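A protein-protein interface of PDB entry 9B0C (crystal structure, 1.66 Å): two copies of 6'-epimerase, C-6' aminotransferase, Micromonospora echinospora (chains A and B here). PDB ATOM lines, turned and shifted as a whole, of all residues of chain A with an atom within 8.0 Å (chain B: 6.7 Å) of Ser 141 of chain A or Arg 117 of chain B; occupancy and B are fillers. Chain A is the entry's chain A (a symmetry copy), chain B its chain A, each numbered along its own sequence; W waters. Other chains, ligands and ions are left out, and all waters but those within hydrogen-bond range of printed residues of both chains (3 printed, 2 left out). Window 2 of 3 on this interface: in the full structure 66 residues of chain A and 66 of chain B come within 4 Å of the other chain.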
ATOM      1  N   ARG A 104      30.097 -40.213  -5.699  1.00  0.00           N
ATOM      2  CA  ARG A 104      30.661 -38.863  -5.589  1.00  0.00           C
ATOM      3  C   ARG A 104      31.757 -38.645  -6.622  1.00  0.00           C
ATOM      4  O   ARG A 104      31.880 -37.553  -7.181  1.00  0.00           O
ATOM      5  CB  ARG A 104      31.225 -38.597  -4.183  1.00  0.00           C
ATOM      6  CG  ARG A 104      32.016 -37.282  -4.090  1.00  0.00           C
ATOM      7  CD  ARG A 104      31.851 -36.589  -2.740  1.00  0.00           C
ATOM      8  NE  ARG A 104      32.725 -35.417  -2.672  1.00  0.00           N
ATOM      9  CZ  ARG A 104      32.336 -34.177  -2.936  1.00  0.00           C
ATOM     10  NH1 ARG A 104      31.097 -33.904  -3.314  1.00  0.00           N
ATOM     11  NH2 ARG A 104      33.212 -33.177  -2.804  1.00  0.00           N
ATOM     12  N   ARG A 111      31.351 -32.763 -13.102  1.00  0.00           N
ATOM     13  CA  ARG A 111      31.624 -31.364 -12.798  1.00  0.00           C
ATOM     14  C   ARG A 111      32.934 -30.901 -13.431  1.00  0.00           C
ATOM     15  O   ARG A 111      33.001 -29.798 -13.987  1.00  0.00           O
ATOM     16  CB  ARG A 111      31.628 -31.167 -11.282  1.00  0.00           C
ATOM     17  CG  ARG A 111      30.225 -31.235 -10.690  1.00  0.00           C
ATOM     18  CD  ARG A 111      30.253 -31.126  -9.179  1.00  0.00           C
ATOM     19  NE  ARG A 111      28.925 -30.895  -8.632  1.00  0.00           N
ATOM     20  CZ  ARG A 111      28.636 -30.911  -7.340  1.00  0.00           C
ATOM     21  NH1 ARG A 111      29.532 -31.297  -6.436  1.00  0.00           N
ATOM     22  NH2 ARG A 111      27.422 -30.537  -6.942  1.00  0.00           N
ATOM     23  N   ARG A 117      28.113 -27.169 -12.015  1.00  0.00           N
ATOM     24  CA  ARG A 117      28.063 -27.662 -10.640  1.00  0.00           C
ATOM     25  C   ARG A 117      26.787 -28.405 -10.298  1.00  0.00           C
ATOM     26  O   ARG A 117      26.846 -29.469  -9.673  1.00  0.00           O
ATOM     27  CB  ARG A 117      28.250 -26.492  -9.661  1.00  0.00           C
ATOM     28  CG  ARG A 117      27.983 -26.882  -8.215  1.00  0.00           C
ATOM     29  CD  ARG A 117      28.982 -26.320  -7.269  1.00  0.00           C
ATOM     30  NE  ARG A 117      28.778 -26.838  -5.922  1.00  0.00           N
ATOM     31  CZ  ARG A 117      29.664 -27.584  -5.276  1.00  0.00           C
ATOM     32  NH1 ARG A 117      30.789 -27.975  -5.857  1.00  0.00           N
ATOM     33  NH2 ARG A 117      29.421 -27.935  -4.015  1.00  0.00           N
ATOM     34  N   ASP A 128      27.019 -39.544   1.689  1.00  0.00           N
ATOM     35  CA  ASP A 128      27.650 -38.227   1.629  1.00  0.00           C
ATOM     36  C   ASP A 128      26.590 -37.138   1.683  1.00  0.00           C
ATOM     37  O   ASP A 128      25.458 -37.325   1.224  1.00  0.00           O
ATOM     38  CB  ASP A 128      28.467 -38.090   0.343  1.00  0.00           C
ATOM     39  CG  ASP A 128      29.387 -36.891   0.356  1.00  0.00           C
ATOM     40  OD1 ASP A 128      30.511 -37.006   0.872  1.00  0.00           O
ATOM     41  OD2 ASP A 128      28.988 -35.829  -0.178  1.00  0.00           O
ATOM     42  N   LEU A 129      26.965 -35.983   2.244  1.00  0.00           N
ATOM     43  CA  LEU A 129      26.013 -34.878   2.295  1.00  0.00           C
ATOM     44  C   LEU A 129      25.536 -34.487   0.908  1.00  0.00           C
ATOM     45  O   LEU A 129      24.437 -33.935   0.776  1.00  0.00           O
ATOM     46  CB  LEU A 129      26.626 -33.658   2.994  1.00  0.00           C
ATOM     47  CG  LEU A 129      26.649 -33.785   4.514  1.00  0.00           C
ATOM     48  CD1 LEU A 129      27.112 -32.461   5.111  1.00  0.00           C
ATOM     49  CD2 LEU A 129      25.279 -34.196   5.011  1.00  0.00           C
ATOM     50  N   MET A 130      26.327 -34.744  -0.134  1.00  0.00           N
ATOM     51  CA  MET A 130      25.853 -34.349  -1.454  1.00  0.00           C
ATOM     52  C   MET A 130      24.644 -35.160  -1.875  1.00  0.00           C
ATOM     53  O   MET A 130      23.899 -34.727  -2.763  1.00  0.00           O
ATOM     54  CB  MET A 130      26.956 -34.471  -2.505  1.00  0.00           C
ATOM     55  CG  MET A 130      27.309 -35.894  -2.935  1.00  0.00           C
ATOM     56  SD  MET A 130      28.492 -35.852  -4.289  1.00  0.00           S
ATOM     57  CE  MET A 130      27.748 -34.678  -5.455  1.00  0.00           C
ATOM     58  N   TRP A 131      24.409 -36.312  -1.249  1.00  0.00           N
ATOM     59  CA  TRP A 131      23.268 -37.127  -1.634  1.00  0.00           C
ATOM     60  C   TRP A 131      22.105 -37.007  -0.661  1.00  0.00           C
ATOM     61  O   TRP A 131      21.130 -37.760  -0.781  1.00  0.00           O
ATOM     62  CB  TRP A 131      23.693 -38.587  -1.790  1.00  0.00           C
ATOM     63  CG  TRP A 131      24.803 -38.786  -2.807  1.00  0.00           C
ATOM     64  CD1 TRP A 131      25.934 -39.523  -2.627  1.00  0.00           C
ATOM     65  CD2 TRP A 131      24.872 -38.277  -4.161  1.00  0.00           C
ATOM     66  NE1 TRP A 131      26.703 -39.506  -3.765  1.00  0.00           N
ATOM     67  CE2 TRP A 131      26.075 -38.759  -4.726  1.00  0.00           C
ATOM     68  CE3 TRP A 131      24.028 -37.481  -4.951  1.00  0.00           C
ATOM     69  CZ2 TRP A 131      26.477 -38.457  -6.027  1.00  0.00           C
ATOM     70  CZ3 TRP A 131      24.427 -37.187  -6.255  1.00  0.00           C
ATOM     71  CH2 TRP A 131      25.646 -37.675  -6.780  1.00  0.00           C
ATOM     72  N   GLU A 132      22.173 -36.059   0.279  1.00  0.00           N
ATOM     73  CA  GLU A 132      21.077 -35.829   1.216  1.00  0.00           C
ATOM     74  C   GLU A 132      19.827 -35.357   0.484  1.00  0.00           C
ATOM     75  O   GLU A 132      19.865 -34.383  -0.271  1.00  0.00           O
ATOM     76  CB  GLU A 132      21.503 -34.791   2.250  1.00  0.00           C
ATOM     77  CG  GLU A 132      20.405 -34.436   3.251  1.00  0.00           C
ATOM     78  CD  GLU A 132      20.875 -33.418   4.282  1.00  0.00           C
ATOM     79  OE1 GLU A 132      21.722 -32.562   3.948  1.00  0.00           O
ATOM     80  OE2 GLU A 132      20.389 -33.480   5.425  1.00  0.00           O
ATOM     81  N   THR A 134      16.457 -33.539  -0.356  1.00  0.00           N
ATOM     82  CA  THR A 134      15.721 -32.322  -0.055  1.00  0.00           C
ATOM     83  C   THR A 134      14.459 -32.323  -0.911  1.00  0.00           C
ATOM     84  O   THR A 134      14.357 -33.091  -1.876  1.00  0.00           O
ATOM     85  CB  THR A 134      16.584 -31.076  -0.344  1.00  0.00           C
ATOM     86  OG1 THR A 134      17.307 -31.244  -1.569  1.00  0.00           O
ATOM     87  CG2 THR A 134      17.601 -30.852   0.778  1.00  0.00           C
ATOM     88  N   GLN A 138      14.388 -27.899  -4.432  1.00  0.00           N
ATOM     89  CA  GLN A 138      15.251 -27.299  -3.424  1.00  0.00           C
ATOM     90  C   GLN A 138      16.633 -27.936  -3.488  1.00  0.00           C
ATOM     91  O   GLN A 138      16.788 -29.097  -3.083  1.00  0.00           O
ATOM     92  CB  GLN A 138      14.632 -27.481  -2.036  1.00  0.00           C
ATOM     93  CG  GLN A 138      13.130 -27.105  -1.984  1.00  0.00           C
ATOM     94  CD  GLN A 138      12.592 -26.975  -0.564  1.00  0.00           C
ATOM     95  OE1 GLN A 138      13.321 -27.178   0.417  1.00  0.00           O
ATOM     96  NE2 GLN A 138      11.320 -26.619  -0.448  1.00  0.00           N
ATOM     97  N   PRO A 139      17.653 -27.238  -3.982  1.00  0.00           N
ATOM     98  CA  PRO A 139      19.002 -27.824  -3.996  1.00  0.00           C
ATOM     99  C   PRO A 139      19.503 -28.052  -2.583  1.00  0.00           C
ATOM    100  O   PRO A 139      19.268 -27.243  -1.681  1.00  0.00           O
ATOM    101  CB  PRO A 139      19.849 -26.772  -4.723  1.00  0.00           C
ATOM    102  CG  PRO A 139      18.857 -25.861  -5.400  1.00  0.00           C
ATOM    103  CD  PRO A 139      17.645 -25.870  -4.517  1.00  0.00           C
ATOM    104  N   ASN A 140      20.201 -29.163  -2.377  1.00  0.00           N
ATOM    105  CA  ASN A 140      20.767 -29.405  -1.060  1.00  0.00           C
ATOM    106  C   ASN A 140      22.080 -28.638  -0.907  1.00  0.00           C
ATOM    107  O   ASN A 140      22.472 -27.835  -1.759  1.00  0.00           O
ATOM    108  CB  ASN A 140      20.904 -30.905  -0.799  1.00  0.00           C
ATOM    109  CG  ASN A 140      21.985 -31.579  -1.629  1.00  0.00           C
ATOM    110  OD1 ASN A 140      22.844 -30.940  -2.244  1.00  0.00           O
ATOM    111  ND2 ASN A 140      21.940 -32.917  -1.643  1.00  0.00           N
ATOM    112  N   SER A 141      22.777 -28.876   0.204  1.00  0.00           N
ATOM    113  CA  SER A 141      23.937 -28.061   0.543  1.00  0.00           C
ATOM    114  C   SER A 141      25.087 -28.237  -0.435  1.00  0.00           C
ATOM    115  O   SER A 141      26.011 -27.419  -0.426  1.00  0.00           O
ATOM    116  CB  SER A 141      24.414 -28.389   1.956  1.00  0.00           C
ATOM    117  OG  SER A 141      25.013 -29.679   2.011  1.00  0.00           O
ATOM    118  N   GLU A 142      25.057 -29.282  -1.267  1.00  0.00           N
ATOM    119  CA  GLU A 142      26.090 -29.517  -2.262  1.00  0.00           C
ATOM    120  C   GLU A 142      25.563 -29.344  -3.684  1.00  0.00           C
ATOM    121  O   GLU A 142      26.150 -29.881  -4.621  1.00  0.00           O
ATOM    122  CB  GLU A 142      26.676 -30.918  -2.087  1.00  0.00           C
ATOM    123  CG  GLU A 142      27.427 -31.166  -0.764  1.00  0.00           C
ATOM    124  CD  GLU A 142      28.726 -30.367  -0.623  1.00  0.00           C
ATOM    125  OE1 GLU A 142      29.103 -29.612  -1.545  1.00  0.00           O
ATOM    126  OE2 GLU A 142      29.416 -30.543   0.400  1.00  0.00           O
ATOM    127  N   ASP A 143      24.447 -28.632  -3.849  1.00  0.00           N
ATOM    128  CA  ASP A 143      23.908 -28.270  -5.165  1.00  0.00           C
ATOM    129  C   ASP A 143      23.439 -29.493  -5.942  1.00  0.00           C
ATOM    130  O   ASP A 143      23.699 -29.636  -7.146  1.00  0.00           O
ATOM    131  CB  ASP A 143      24.918 -27.458  -5.970  1.00  0.00           C
ATOM    132  CG  ASP A 143      25.232 -26.149  -5.299  1.00  0.00           C
ATOM    133  OD1 ASP A 143      24.256 -25.460  -4.936  1.00  0.00           O
ATOM    134  OD2 ASP A 143      26.421 -25.831  -5.109  1.00  0.00           O
ATOM    135  N   VAL A 144      22.738 -30.378  -5.245  1.00  0.00           N
ATOM    136  CA  VAL A 144      22.071 -31.518  -5.858  1.00  0.00           C
ATOM    137  C   VAL A 144      20.566 -31.330  -5.709  1.00  0.00           C
ATOM    138  O   VAL A 144      20.079 -31.012  -4.617  1.00  0.00           O
ATOM    139  CB  VAL A 144      22.541 -32.841  -5.228  1.00  0.00           C
ATOM    140  CG1 VAL A 144      21.761 -34.043  -5.815  1.00  0.00           C
ATOM    141  CG2 VAL A 144      24.032 -33.002  -5.432  1.00  0.00           C
ATOM    142  N   HIS A 146      16.764 -33.197  -6.266  1.00  0.00           N
ATOM    143  CA  HIS A 146      16.195 -34.539  -6.209  1.00  0.00           C
ATOM    144  C   HIS A 146      14.858 -34.586  -6.937  1.00  0.00           C
ATOM    145  O   HIS A 146      13.998 -33.732  -6.702  1.00  0.00           O
ATOM    146  CB  HIS A 146      16.058 -34.974  -4.756  1.00  0.00           C
ATOM    147  CG  HIS A 146      17.375 -35.017  -4.050  1.00  0.00           C
ATOM    148  ND1 HIS A 146      18.148 -36.159  -3.997  1.00  0.00           N
ATOM    149  CD2 HIS A 146      18.083 -34.050  -3.420  1.00  0.00           C
ATOM    150  CE1 HIS A 146      19.267 -35.896  -3.345  1.00  0.00           C
ATOM    151  NE2 HIS A 146      19.255 -34.622  -2.989  1.00  0.00           N
ATOM    152  N   ARG B 104      36.845 -36.004   4.832  1.00  0.00           N
ATOM    153  CA  ARG B 104      35.631 -35.346   4.335  1.00  0.00           C
ATOM    154  C   ARG B 104      34.501 -35.455   5.348  1.00  0.00           C
ATOM    155  O   ARG B 104      33.719 -34.517   5.516  1.00  0.00           O
ATOM    156  CB  ARG B 104      35.173 -35.939   2.992  1.00  0.00           C
ATOM    157  CG  ARG B 104      33.792 -35.431   2.549  1.00  0.00           C
ATOM    158  CD  ARG B 104      33.681 -35.271   1.035  1.00  0.00           C
ATOM    159  NE  ARG B 104      32.310 -34.908   0.671  1.00  0.00           N
ATOM    160  CZ  ARG B 104      31.895 -33.667   0.459  1.00  0.00           C
ATOM    161  NH1 ARG B 104      32.711 -32.631   0.585  1.00  0.00           N
ATOM    162  NH2 ARG B 104      30.628 -33.457   0.094  1.00  0.00           N
ATOM    163  N   ALA B 107      35.085 -32.904   8.102  1.00  0.00           N
ATOM    164  CA  ALA B 107      34.745 -31.574   7.611  1.00  0.00           C
ATOM    165  C   ALA B 107      33.242 -31.397   7.522  1.00  0.00           C
ATOM    166  O   ALA B 107      32.714 -30.327   7.858  1.00  0.00           O
ATOM    167  CB  ALA B 107      35.384 -31.322   6.243  1.00  0.00           C
ATOM    168  N   ARG B 111      30.790 -28.621   9.383  1.00  0.00           N
ATOM    169  CA  ARG B 111      29.806 -27.827   8.657  1.00  0.00           C
ATOM    170  C   ARG B 111      28.405 -28.009   9.236  1.00  0.00           C
ATOM    171  O   ARG B 111      27.664 -27.031   9.391  1.00  0.00           O
ATOM    172  CB  ARG B 111      29.856 -28.192   7.173  1.00  0.00           C
ATOM    173  CG  ARG B 111      31.105 -27.647   6.489  1.00  0.00           C
ATOM    174  CD  ARG B 111      31.185 -28.089   5.043  1.00  0.00           C
ATOM    175  NE  ARG B 111      32.198 -27.347   4.309  1.00  0.00           N
ATOM    176  CZ  ARG B 111      32.584 -27.630   3.074  1.00  0.00           C
ATOM    177  NH1 ARG B 111      32.170 -28.733   2.456  1.00  0.00           N
ATOM    178  NH2 ARG B 111      33.407 -26.795   2.443  1.00  0.00           N
ATOM    179  N   GLN B 112      28.028 -29.245   9.584  1.00  0.00           N
ATOM    180  CA  GLN B 112      26.673 -29.465  10.098  1.00  0.00           C
ATOM    181  C   GLN B 112      26.476 -28.784  11.445  1.00  0.00           C
ATOM    182  O   GLN B 112      25.436 -28.158  11.691  1.00  0.00           O
ATOM    183  CB  GLN B 112      26.390 -30.966  10.206  1.00  0.00           C
ATOM    184  CG  GLN B 112      26.306 -31.662   8.842  1.00  0.00           C
ATOM    185  CD  GLN B 112      24.977 -31.450   8.159  1.00  0.00           C
ATOM    186  OE1 GLN B 112      24.760 -30.434   7.483  1.00  0.00           O
ATOM    187  NE2 GLN B 112      24.071 -32.410   8.330  1.00  0.00           N
ATOM    188  N   THR B 114      28.263 -26.224  12.880  1.00  0.00           N
ATOM    189  CA  THR B 114      28.433 -24.775  12.891  1.00  0.00           C
ATOM    190  C   THR B 114      27.461 -24.054  11.968  1.00  0.00           C
ATOM    191  O   THR B 114      27.259 -22.847  12.132  1.00  0.00           O
ATOM    192  CB  THR B 114      29.850 -24.393  12.462  1.00  0.00           C
ATOM    193  OG1 THR B 114      30.061 -24.823  11.108  1.00  0.00           O
ATOM    194  CG2 THR B 114      30.895 -25.032  13.395  1.00  0.00           C
ATOM    195  N   GLY B 115      26.892 -24.746  10.985  1.00  0.00           N
ATOM    196  CA  GLY B 115      26.132 -24.068   9.950  1.00  0.00           C
ATOM    197  C   GLY B 115      26.947 -23.188   9.032  1.00  0.00           C
ATOM    198  O   GLY B 115      26.373 -22.364   8.313  1.00  0.00           O
ATOM    199  N   LYS B 116      28.268 -23.321   9.046  1.00  0.00           N
ATOM    200  CA  LYS B 116      29.172 -22.572   8.189  1.00  0.00           C
ATOM    201  C   LYS B 116      29.753 -23.516   7.148  1.00  0.00           C
ATOM    202  O   LYS B 116      29.611 -24.735   7.250  1.00  0.00           O
ATOM    203  CB  LYS B 116      30.280 -21.907   9.014  1.00  0.00           C
ATOM    204  CG  LYS B 116      29.718 -21.027  10.127  1.00  0.00           C
ATOM    205  CD  LYS B 116      30.800 -20.477  11.042  1.00  0.00           C
ATOM    206  CE  LYS B 116      30.164 -19.608  12.125  1.00  0.00           C
ATOM    207  NZ  LYS B 116      31.090 -19.304  13.256  1.00  0.00           N
ATOM    208  N   ARG B 117      30.379 -22.947   6.129  1.00  0.00           N
ATOM    209  CA  ARG B 117      30.849 -23.752   5.003  1.00  0.00           C
ATOM    210  C   ARG B 117      32.350 -23.701   4.795  1.00  0.00           C
ATOM    211  O   ARG B 117      32.973 -24.746   4.576  1.00  0.00           O
ATOM    212  CB  ARG B 117      30.140 -23.308   3.715  1.00  0.00           C
ATOM    213  CG  ARG B 117      30.736 -23.937   2.464  1.00  0.00           C
ATOM    214  CD  ARG B 117      29.706 -24.400   1.499  1.00  0.00           C
ATOM    215  NE  ARG B 117      30.313 -25.127   0.392  1.00  0.00           N
ATOM    216  CZ  ARG B 117      30.083 -26.408   0.136  1.00  0.00           C
ATOM    217  NH1 ARG B 117      29.323 -27.144   0.933  1.00  0.00           N
ATOM    218  NH2 ARG B 117      30.618 -26.958  -0.953  1.00  0.00           N
ATOM    219  N   LEU B 118      32.952 -22.517   4.856  1.00  0.00           N
ATOM    220  CA  LEU B 118      34.372 -22.369   4.577  1.00  0.00           C
ATOM    221  C   LEU B 118      35.216 -23.217   5.525  1.00  0.00           C
ATOM    222  O   LEU B 118      34.941 -23.301   6.725  1.00  0.00           O
ATOM    223  CB  LEU B 118      34.753 -20.894   4.713  1.00  0.00           C
ATOM    224  CG  LEU B 118      36.022 -20.375   4.054  1.00  0.00           C
ATOM    225  CD1 LEU B 118      35.956 -20.476   2.531  1.00  0.00           C
ATOM    226  CD2 LEU B 118      36.272 -18.929   4.496  1.00  0.00           C
ATOM    227  N   ILE B 119      36.246 -23.844   4.971  1.00  0.00           N
ATOM    228  CA  ILE B 119      37.205 -24.659   5.719  1.00  0.00           C
ATOM    229  C   ILE B 119      38.602 -24.147   5.398  1.00  0.00           C
ATOM    230  O   ILE B 119      38.905 -23.852   4.236  1.00  0.00           O
ATOM    231  CB  ILE B 119      37.071 -26.152   5.331  1.00  0.00           C
ATOM    232  CG1 ILE B 119      35.670 -26.704   5.647  1.00  0.00           C
ATOM    233  CG2 ILE B 119      38.222 -27.021   5.948  1.00  0.00           C
ATOM    234  CD1 ILE B 119      35.514 -27.325   6.976  1.00  0.00           C
ATOM    235  N   SER B 141      37.036 -25.319  -5.305  1.00  0.00           N
ATOM    236  CA  SER B 141      35.664 -25.479  -5.771  1.00  0.00           C
ATOM    237  C   SER B 141      34.718 -25.933  -4.671  1.00  0.00           C
ATOM    238  O   SER B 141      33.501 -25.845  -4.854  1.00  0.00           O
ATOM    239  CB  SER B 141      35.614 -26.472  -6.930  1.00  0.00           C
ATOM    240  OG  SER B 141      35.862 -27.799  -6.481  1.00  0.00           O
ATOM    241  N   GLU B 142      35.244 -26.421  -3.545  1.00  0.00           N
ATOM    242  CA  GLU B 142      34.426 -26.849  -2.422  1.00  0.00           C
ATOM    243  C   GLU B 142      34.603 -25.942  -1.208  1.00  0.00           C
ATOM    244  O   GLU B 142      34.326 -26.362  -0.087  1.00  0.00           O
ATOM    245  CB  GLU B 142      34.761 -28.293  -2.050  1.00  0.00           C
ATOM    246  CG  GLU B 142      34.433 -29.351  -3.122  1.00  0.00           C
ATOM    247  CD  GLU B 142      32.934 -29.535  -3.381  1.00  0.00           C
ATOM    248  OE1 GLU B 142      32.098 -28.871  -2.732  1.00  0.00           O
ATOM    249  OE2 GLU B 142      32.583 -30.403  -4.203  1.00  0.00           O
ATOM    250  N   ASP B 143      35.092 -24.717  -1.416  1.00  0.00           N
ATOM    251  CA  ASP B 143      35.183 -23.696  -0.365  1.00  0.00           C
ATOM    252  C   ASP B 143      36.175 -24.088   0.722  1.00  0.00           C
ATOM    253  O   ASP B 143      35.913 -23.938   1.925  1.00  0.00           O
ATOM    254  CB  ASP B 143      33.811 -23.388   0.224  1.00  0.00           C
ATOM    255  CG  ASP B 143      32.885 -22.808  -0.809  1.00  0.00           C
ATOM    256  OD1 ASP B 143      33.330 -21.859  -1.488  1.00  0.00           O
ATOM    257  OD2 ASP B 143      31.755 -23.308  -0.965  1.00  0.00           O
ATOM    258  N   VAL B 144      37.324 -24.591   0.292  1.00  0.00           N
ATOM    259  CA  VAL B 144      38.449 -24.863   1.177  1.00  0.00           C
ATOM    260  C   VAL B 144      39.587 -23.918   0.810  1.00  0.00           C
ATOM    261  O   VAL B 144      39.924 -23.771  -0.373  1.00  0.00           O
ATOM    262  CB  VAL B 144      38.884 -26.336   1.083  1.00  0.00           C
ATOM    263  CG1 VAL B 144      40.139 -26.600   1.952  1.00  0.00           C
ATOM    264  CG2 VAL B 144      37.737 -27.234   1.492  1.00  0.00           C
ATOM    265  N   GLU B 164      33.423 -17.070   9.948  1.00  0.00           N
ATOM    266  CA  GLU B 164      32.647 -17.892   9.024  1.00  0.00           C
ATOM    267  C   GLU B 164      33.333 -19.210   8.683  1.00  0.00           C
ATOM    268  O   GLU B 164      32.895 -19.895   7.749  1.00  0.00           O
ATOM    269  CB  GLU B 164      32.356 -17.121   7.736  1.00  0.00           C
ATOM    270  CG  GLU B 164      33.492 -16.242   7.288  1.00  0.00           C
ATOM    271  CD  GLU B 164      33.163 -15.462   6.032  1.00  0.00           C
ATOM    272  OE1 GLU B 164      31.977 -15.455   5.631  1.00  0.00           O
ATOM    273  OE2 GLU B 164      34.090 -14.849   5.456  1.00  0.00           O
ATOM    274  N   LEU B 165      34.394 -19.570   9.395  1.00  0.00           N
ATOM    275  CA  LEU B 165      35.043 -20.856   9.170  1.00  0.00           C
ATOM    276  C   LEU B 165      34.279 -21.935   9.916  1.00  0.00           C
ATOM    277  O   LEU B 165      33.978 -21.786  11.105  1.00  0.00           O
ATOM    278  CB  LEU B 165      36.491 -20.833   9.655  1.00  0.00           C
ATOM    279  CG  LEU B 165      37.522 -20.120   8.794  1.00  0.00           C
ATOM    280  CD1 LEU B 165      38.872 -20.048   9.531  1.00  0.00           C
ATOM    281  CD2 LEU B 165      37.646 -20.794   7.422  1.00  0.00           C
ATOM    282  N   ALA B 166      33.965 -23.021   9.215  1.00  0.00           N
ATOM    283  CA  ALA B 166      33.421 -24.191   9.888  1.00  0.00           C
ATOM    284  C   ALA B 166      34.494 -24.912  10.691  1.00  0.00           C
ATOM    285  O   ALA B 166      34.201 -25.453  11.762  1.00  0.00           O
ATOM    286  CB  ALA B 166      32.808 -25.144   8.860  1.00  0.00           C
ATOM    287  N   ALA B 167      35.725 -24.933  10.189  1.00  0.00           N
ATOM    288  CA  ALA B 167      36.805 -25.657  10.849  1.00  0.00           C
ATOM    289  C   ALA B 167      38.118 -25.381  10.149  1.00  0.00           C
ATOM    290  O   ALA B 167      38.153 -24.935   8.998  1.00  0.00           O
ATOM    291  CB  ALA B 167      36.558 -27.171  10.852  1.00  0.00           C
HETATM  292  O   HOH W   1      30.000 -30.811   3.124  1.00  0.00           O
HETATM  293  O   HOH W   2      22.664 -30.548   5.662  1.00  0.00           O
HETATM  294  O   HOH W   3      32.555 -31.853  -6.597  1.00  0.00           O
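The side-chain carboxylate (OD1) of Asp 128 of chain A lies within salt-bridge range of the guanidinium group (NE) of Arg 104 of chain B (2.8 Å). OE2 of Glu 142 of chain A lies within salt-bridge range of NH2 of Arg 104 of chain B, at 3.2 Å. OE2 of Glu 142 of chain A is in salt-bridge range of NH1 of Arg 111 of chain B (3.9 Å). The guanidinium group (NH2) of Arg 117 of chain B lies within salt-bridge range of the side-chain carboxylate (OE1) of Glu 142 of chain A (3.1 Å). NH2 of Arg 104 of chain A lies within salt-bridge range of OE2 of Glu 142 of chain B (3.2 Å). The side-chain carboxylate of Glu 142 of chain B is in salt-bridge range of the guanidinium group of Arg 111 of chain A (3.9 Å). OE1 of Glu 142 of chain B is in salt-bridge range of NH2 of Arg 117 of chain A (3.1 Å). The guanidinium group (NE) of Arg 104 of chain A lies close to the guanidinium group (NE) of Arg 104 of chain B (3.4 Å). The guanidinium group of Arg 117 of chain A lies close to the guanidinium group of Arg 117 of chain B, 3.4 Å away. OE1 of Glu 142 of chain B sits close to OE1 of Glu 142 of chain A (3.3 Å).
Of the 17 printed residues of chain A, 7 touch a printed residue of chain B. Hydrophobic or aromatic side chains of chain A within 4 Å of the printed part of chain B: Leu 129. Along chain A the printed residues that touch a printed residue of chain B span positions 104 to 142. Of the 18 printed residues of chain B, 6 touch a printed residue of chain A. Printed residues of chain B that touch a printed residue of chain A: Arg 104, Arg 111, Gln 112, Arg 117, Ser 141 and Glu 142. Among the printed residues, 13 pairs touch across the chains.
Of the printed residues of chain B, Arg 117 of chain A touches Arg 117 (3.4 Å), Ser 141 (3.6 Å) and Glu 142 (3.1 Å). Asn 140 of chain A touches none of the printed residues of chain B. Ser 141 of chain A touches just one residue of chain B: Arg 117 (3.6 Å). Of the printed residues of chain A, Arg 111 of chain B touches Glu 142 (3.9 Å). Arg 117 of chain B touches just these residues of chain A: Arg 117 (3.4 Å), Ser 141 (3.6 Å) and Glu 142 (3.1 Å). Of the printed residues of chain A, Ser 141 of chain B touches Arg 117 (3.6 Å). Printed residues of chain A within 4 Å of Glu 142 of chain B: Arg 104 (3.2 Å), Arg 111 (3.9 Å), Arg 117 (3.1 Å) and Glu 142 (3.3 Å). The nearest residue of chain B that does not touch Ser 141 of chain A is Gln 112 of chain B (5.5 Å). The nearest printed residue of chain B that does not touch Arg 111 of chain A is Ser 141 of chain B (6.9 Å).
The guanidinium group of Arg 111 of chain B sits at hydrogen-bond distance from the backbone carbonyl oxygen of Arg 117 of chain B (2.7 Å). The side-chain carboxylate (OE1) of Glu 142 of chain B is in salt-bridge range of the guanidinium group (NH2) of Arg 117 of chain B. The guanidinium group (NE) of Arg 117 of chain B lies within salt-bridge range of the side-chain carboxylate (OD2) of Asp 143 of chain B (2.7 Å).
Water W2 lies within hydrogen-bond range of the side-chain amide oxygen (OE1) of Gln 112 of chain B (2.8 Å) and the side-chain carboxylate (OE1) of Glu 132 of chain A (2.8 Å). Water W3 bridges OE2 of Glu 142 of chain B (2.8 Å) and NH1 of Arg 111 of chain A (3.1 Å). Water W1 lies within hydrogen-bond range of OE2 of Glu 142 of chain A and NH1 of Arg 111 of chain B.
Arg 104 of chain A touches Glu 142 of chain B, and with the chains exchanged Glu 142 of chain A touches Arg 104 of chain B. Arg 111 of chain A touches Glu 142 of chain B, and with the chains exchanged Glu 142 of chain A touches Arg 111 of chain B. Arg 117 of chain A touches its own counterpart, Arg 117 of chain B. Arg 117 of chain A touches Glu 142 of chain B, and with the chains exchanged Glu 142 of chain A touches Arg 117 of chain B.
NH1 of Arg 117 of chain A touches O of Ser 141 of chain B (3.6 Å). Gln 112 of chain B touches Leu 129 of chain A. Ser 141 of chain A touches Arg 117 of chain B.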
